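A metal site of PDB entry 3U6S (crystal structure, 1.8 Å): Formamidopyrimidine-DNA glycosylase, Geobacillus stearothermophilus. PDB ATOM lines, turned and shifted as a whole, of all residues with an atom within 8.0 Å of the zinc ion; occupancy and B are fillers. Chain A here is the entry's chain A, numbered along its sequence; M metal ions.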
ATOM      1  N   PHE A 181     -13.492 -10.244 -26.770  1.00  0.00           N
ATOM      2  CA  PHE A 181     -13.598 -11.419 -25.904  1.00  0.00           C
ATOM      3  C   PHE A 181     -14.661 -11.196 -24.819  1.00  0.00           C
ATOM      4  O   PHE A 181     -15.524 -12.052 -24.595  1.00  0.00           O
ATOM      5  CB  PHE A 181     -12.269 -11.788 -25.259  1.00  0.00           C
ATOM      6  CG  PHE A 181     -12.393 -12.854 -24.199  1.00  0.00           C
ATOM      7  CD1 PHE A 181     -12.423 -14.204 -24.560  1.00  0.00           C
ATOM      8  CD2 PHE A 181     -12.548 -12.517 -22.864  1.00  0.00           C
ATOM      9  CE1 PHE A 181     -12.562 -15.183 -23.587  1.00  0.00           C
ATOM     10  CE2 PHE A 181     -12.702 -13.489 -21.892  1.00  0.00           C
ATOM     11  CZ  PHE A 181     -12.708 -14.825 -22.243  1.00  0.00           C
ATOM     12  N   TYR A 239      -7.299 -11.413 -20.997  1.00  0.00           N
ATOM     13  CA  TYR A 239      -8.004 -12.655 -21.287  1.00  0.00           C
ATOM     14  C   TYR A 239      -7.459 -13.361 -22.528  1.00  0.00           C
ATOM     15  O   TYR A 239      -7.387 -14.588 -22.567  1.00  0.00           O
ATOM     16  CB  TYR A 239      -9.488 -12.367 -21.504  1.00  0.00           C
ATOM     17  CG  TYR A 239     -10.218 -11.955 -20.264  1.00  0.00           C
ATOM     18  CD1 TYR A 239     -10.625 -10.643 -20.079  1.00  0.00           C
ATOM     19  CD2 TYR A 239     -10.504 -12.881 -19.272  1.00  0.00           C
ATOM     20  CE1 TYR A 239     -11.297 -10.254 -18.927  1.00  0.00           C
ATOM     21  CE2 TYR A 239     -11.172 -12.511 -18.125  1.00  0.00           C
ATOM     22  CZ  TYR A 239     -11.574 -11.203 -17.956  1.00  0.00           C
ATOM     23  OH  TYR A 239     -12.239 -10.843 -16.813  1.00  0.00           O
ATOM     24  N   VAL A 240      -7.114 -12.592 -23.556  1.00  0.00           N
ATOM     25  CA  VAL A 240      -6.720 -13.211 -24.820  1.00  0.00           C
ATOM     26  C   VAL A 240      -5.453 -12.629 -25.440  1.00  0.00           C
ATOM     27  O   VAL A 240      -4.640 -13.367 -25.985  1.00  0.00           O
ATOM     28  CB  VAL A 240      -7.858 -13.188 -25.875  1.00  0.00           C
ATOM     29  CG1 VAL A 240      -9.046 -14.025 -25.412  1.00  0.00           C
ATOM     30  CG2 VAL A 240      -8.286 -11.764 -26.227  1.00  0.00           C
ATOM     31  N   PRO A 247      -4.540 -21.618 -21.910  1.00  0.00           N
ATOM     32  CA  PRO A 247      -5.954 -21.854 -21.640  1.00  0.00           C
ATOM     33  C   PRO A 247      -6.722 -20.542 -21.436  1.00  0.00           C
ATOM     34  O   PRO A 247      -6.256 -19.644 -20.734  1.00  0.00           O
ATOM     35  CB  PRO A 247      -5.935 -22.637 -20.325  1.00  0.00           C
ATOM     36  CG  PRO A 247      -4.562 -23.208 -20.228  1.00  0.00           C
ATOM     37  CD  PRO A 247      -3.669 -22.198 -20.872  1.00  0.00           C
ATOM     38  N   CYS A 248      -7.889 -20.452 -22.055  1.00  0.00           N
ATOM     39  CA  CYS A 248      -8.803 -19.352 -21.770  1.00  0.00           C
ATOM     40  C   CYS A 248      -9.064 -19.325 -20.274  1.00  0.00           C
ATOM     41  O   CYS A 248      -9.244 -20.364 -19.642  1.00  0.00           O
ATOM     42  CB  CYS A 248     -10.112 -19.570 -22.517  1.00  0.00           C
ATOM     43  SG  CYS A 248     -11.399 -18.359 -22.130  1.00  0.00           S
ATOM     44  N   LYS A 249      -9.088 -18.119 -19.692  1.00  0.00           N
ATOM     45  CA  LYS A 249      -9.271 -17.980 -18.256  1.00  0.00           C
ATOM     46  C   LYS A 249     -10.705 -18.246 -17.833  1.00  0.00           C
ATOM     47  O   LYS A 249     -11.009 -18.366 -16.640  1.00  0.00           O
ATOM     48  CB  LYS A 249      -8.824 -16.602 -17.779  1.00  0.00           C
ATOM     49  CG  LYS A 249      -7.327 -16.354 -17.944  1.00  0.00           C
ATOM     50  CD  LYS A 249      -6.928 -14.978 -17.425  1.00  0.00           C
ATOM     51  CE  LYS A 249      -5.433 -14.752 -17.629  1.00  0.00           C
ATOM     52  NZ  LYS A 249      -4.992 -13.403 -17.164  1.00  0.00           N
ATOM     53  N   ARG A 250     -11.605 -18.346 -18.808  1.00  0.00           N
ATOM     54  CA  ARG A 250     -13.021 -18.556 -18.522  1.00  0.00           C
ATOM     55  C   ARG A 250     -13.539 -19.945 -18.917  1.00  0.00           C
ATOM     56  O   ARG A 250     -14.528 -20.403 -18.366  1.00  0.00           O
ATOM     57  CB  ARG A 250     -13.866 -17.454 -19.159  1.00  0.00           C
ATOM     58  CG  ARG A 250     -13.690 -16.113 -18.498  1.00  0.00           C
ATOM     59  CD  ARG A 250     -14.701 -15.100 -18.979  1.00  0.00           C
ATOM     60  NE  ARG A 250     -14.725 -13.921 -18.125  1.00  0.00           N
ATOM     61  CZ  ARG A 250     -15.275 -12.760 -18.455  1.00  0.00           C
ATOM     62  NH1 ARG A 250     -15.848 -12.626 -19.649  1.00  0.00           N
ATOM     63  NH2 ARG A 250     -15.250 -11.746 -17.617  1.00  0.00           N
ATOM     64  N   CYS A 251     -12.885 -20.599 -19.875  1.00  0.00           N
ATOM     65  CA  CYS A 251     -13.341 -21.934 -20.292  1.00  0.00           C
ATOM     66  C   CYS A 251     -12.241 -22.974 -20.474  1.00  0.00           C
ATOM     67  O   CYS A 251     -12.523 -24.161 -20.661  1.00  0.00           O
ATOM     68  CB  CYS A 251     -14.186 -21.838 -21.554  1.00  0.00           C
ATOM     69  SG  CYS A 251     -13.203 -21.638 -23.049  1.00  0.00           S
ATOM     70  N   GLY A 252     -10.980 -22.549 -20.427  1.00  0.00           N
ATOM     71  CA  GLY A 252      -9.871 -23.472 -20.527  1.00  0.00           C
ATOM     72  C   GLY A 252      -9.506 -23.900 -21.952  1.00  0.00           C
ATOM     73  O   GLY A 252      -8.540 -24.627 -22.150  1.00  0.00           O
ATOM     74  N   THR A 253     -10.286 -23.453 -22.934  1.00  0.00           N
ATOM     75  CA  THR A 253      -9.981 -23.756 -24.327  1.00  0.00           C
ATOM     76  C   THR A 253      -8.731 -22.984 -24.732  1.00  0.00           C
ATOM     77  O   THR A 253      -8.596 -21.813 -24.367  1.00  0.00           O
ATOM     78  CB  THR A 253     -11.150 -23.370 -25.255  1.00  0.00           C
ATOM     79  OG1 THR A 253     -12.328 -24.093 -24.879  1.00  0.00           O
ATOM     80  CG2 THR A 253     -10.806 -23.663 -26.720  1.00  0.00           C
ATOM     81  N   PRO A 254      -7.810 -23.614 -25.476  1.00  0.00           N
ATOM     82  CA  PRO A 254      -6.618 -22.860 -25.869  1.00  0.00           C
ATOM     83  C   PRO A 254      -6.965 -21.633 -26.684  1.00  0.00           C
ATOM     84  O   PRO A 254      -7.749 -21.697 -27.646  1.00  0.00           O
ATOM     85  CB  PRO A 254      -5.827 -23.856 -26.721  1.00  0.00           C
ATOM     86  CG  PRO A 254      -6.253 -25.197 -26.221  1.00  0.00           C
ATOM     87  CD  PRO A 254      -7.717 -25.031 -25.867  1.00  0.00           C
ATOM     88  N   ILE A 255      -6.382 -20.502 -26.305  1.00  0.00           N
ATOM     89  CA  ILE A 255      -6.561 -19.257 -27.035  1.00  0.00           C
ATOM     90  C   ILE A 255      -5.891 -19.412 -28.395  1.00  0.00           C
ATOM     91  O   ILE A 255      -4.811 -20.013 -28.519  1.00  0.00           O
ATOM     92  CB  ILE A 255      -5.984 -18.052 -26.258  1.00  0.00           C
ATOM     93  CG1 ILE A 255      -6.737 -17.888 -24.926  1.00  0.00           C
ATOM     94  CG2 ILE A 255      -6.048 -16.757 -27.092  1.00  0.00           C
ATOM     95  CD1 ILE A 255      -8.258 -17.750 -25.103  1.00  0.00           C
ATOM     96  N   TYR A 267      -8.258 -14.707 -29.743  1.00  0.00           N
ATOM     97  CA  TYR A 267      -9.631 -14.967 -29.359  1.00  0.00           C
ATOM     98  C   TYR A 267      -9.769 -16.363 -28.790  1.00  0.00           C
ATOM     99  O   TYR A 267      -8.928 -17.232 -29.009  1.00  0.00           O
ATOM    100  CB  TYR A 267     -10.554 -14.798 -30.573  1.00  0.00           C
ATOM    101  CG  TYR A 267     -10.163 -15.701 -31.716  1.00  0.00           C
ATOM    102  CD1 TYR A 267     -10.776 -16.948 -31.874  1.00  0.00           C
ATOM    103  CD2 TYR A 267      -9.164 -15.342 -32.611  1.00  0.00           C
ATOM    104  CE1 TYR A 267     -10.408 -17.793 -32.910  1.00  0.00           C
ATOM    105  CE2 TYR A 267      -8.791 -16.187 -33.638  1.00  0.00           C
ATOM    106  CZ  TYR A 267      -9.419 -17.410 -33.784  1.00  0.00           C
ATOM    107  OH  TYR A 267      -9.056 -18.250 -34.804  1.00  0.00           O
ATOM    108  N   CYS A 268     -10.844 -16.579 -28.043  1.00  0.00           N
ATOM    109  CA  CYS A 268     -11.204 -17.906 -27.608  1.00  0.00           C
ATOM    110  C   CYS A 268     -12.317 -18.402 -28.519  1.00  0.00           C
ATOM    111  O   CYS A 268     -13.362 -17.758 -28.617  1.00  0.00           O
ATOM    112  CB  CYS A 268     -11.679 -17.887 -26.165  1.00  0.00           C
ATOM    113  SG  CYS A 268     -12.357 -19.462 -25.674  1.00  0.00           S
ATOM    114  N   PRO A 269     -12.094 -19.540 -29.198  1.00  0.00           N
ATOM    115  CA  PRO A 269     -13.062 -20.041 -30.181  1.00  0.00           C
ATOM    116  C   PRO A 269     -14.332 -20.601 -29.531  1.00  0.00           C
ATOM    117  O   PRO A 269     -15.318 -20.852 -30.218  1.00  0.00           O
ATOM    118  CB  PRO A 269     -12.285 -21.143 -30.905  1.00  0.00           C
ATOM    119  CG  PRO A 269     -11.302 -21.630 -29.905  1.00  0.00           C
ATOM    120  CD  PRO A 269     -10.927 -20.433 -29.056  1.00  0.00           C
ATOM    121  N   ARG A 270     -14.302 -20.780 -28.216  1.00  0.00           N
ATOM    122  CA  ARG A 270     -15.483 -21.242 -27.492  1.00  0.00           C
ATOM    123  C   ARG A 270     -16.308 -20.093 -26.898  1.00  0.00           C
ATOM    124  O   ARG A 270     -17.526 -20.041 -27.068  1.00  0.00           O
ATOM    125  CB  ARG A 270     -15.080 -22.239 -26.395  1.00  0.00           C
ATOM    126  CG  ARG A 270     -16.271 -22.777 -25.638  1.00  0.00           C
ATOM    127  CD  ARG A 270     -15.879 -23.789 -24.572  1.00  0.00           C
ATOM    128  NE  ARG A 270     -17.075 -24.323 -23.943  1.00  0.00           N
ATOM    129  CZ  ARG A 270     -17.094 -25.361 -23.105  1.00  0.00           C
ATOM    130  NH1 ARG A 270     -18.245 -25.762 -22.596  1.00  0.00           N
ATOM    131  NH2 ARG A 270     -15.970 -25.988 -22.779  1.00  0.00           N
ATOM    132  N   CYS A 271     -15.641 -19.156 -26.227  1.00  0.00           N
ATOM    133  CA  CYS A 271     -16.321 -18.007 -25.619  1.00  0.00           C
ATOM    134  C   CYS A 271     -16.851 -17.003 -26.632  1.00  0.00           C
ATOM    135  O   CYS A 271     -17.841 -16.311 -26.375  1.00  0.00           O
ATOM    136  CB  CYS A 271     -15.395 -17.268 -24.638  1.00  0.00           C
ATOM    137  SG  CYS A 271     -15.028 -18.169 -23.097  1.00  0.00           S
ATOM    138  N   GLN A 272     -16.186 -16.902 -27.776  1.00  0.00           N
ATOM    139  CA  GLN A 272     -16.567 -15.917 -28.780  1.00  0.00           C
ATOM    140  C   GLN A 272     -17.243 -16.596 -29.965  1.00  0.00           C
ATOM    141  O   GLN A 272     -16.806 -17.651 -30.413  1.00  0.00           O
ATOM    142  CB  GLN A 272     -15.353 -15.120 -29.230  1.00  0.00           C
ATOM    143  CG  GLN A 272     -14.782 -14.241 -28.118  1.00  0.00           C
ATOM    144  CD  GLN A 272     -13.403 -13.700 -28.433  1.00  0.00           C
ATOM    145  OE1 GLN A 272     -12.410 -14.218 -27.936  1.00  0.00           O
ATOM    146  NE2 GLN A 272     -13.354 -12.649 -29.254  1.00  0.00           N
HETATM  147 ZN    ZN M   1     -13.055 -19.297 -23.501  1.00  0.00          ZN
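The zinc ion is bound by the side-chain sulfur (SG) of Cys 268, the side-chain sulfur (SG) of Cys 271, the side-chain sulfur (SG) of Cys 248 and the side-chain sulfur (SG) of Cys 251.
The zinc ion has four donor atoms within binding distance.
The side-chain sulfur (SG) of Cys 268 sits close to the backbone NH (N) of Arg 270 (3.5 Å).
The side-chain sulfur (SG) of Cys 248 sits close to the backbone NH (N) of Arg 250 (3.3 Å).
The side-chain sulfur (SG) of Cys 251 lies close to the side-chain hydroxyl (OG1) of Thr 253, at 3.2 Å.
The backbone NH (N) of Cys 248 lies within hydrogen-bond range of the backbone carbonyl oxygen (O) of Thr 253, at 2.8 Å.
The backbone NH of Cys 268 sits at hydrogen-bond distance from the side-chain amide oxygen of Gln 272 (2.8 Å).
Within 4 Å of the zinc ion: Cys 248, Cys 251, Cys 268 and Cys 271.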
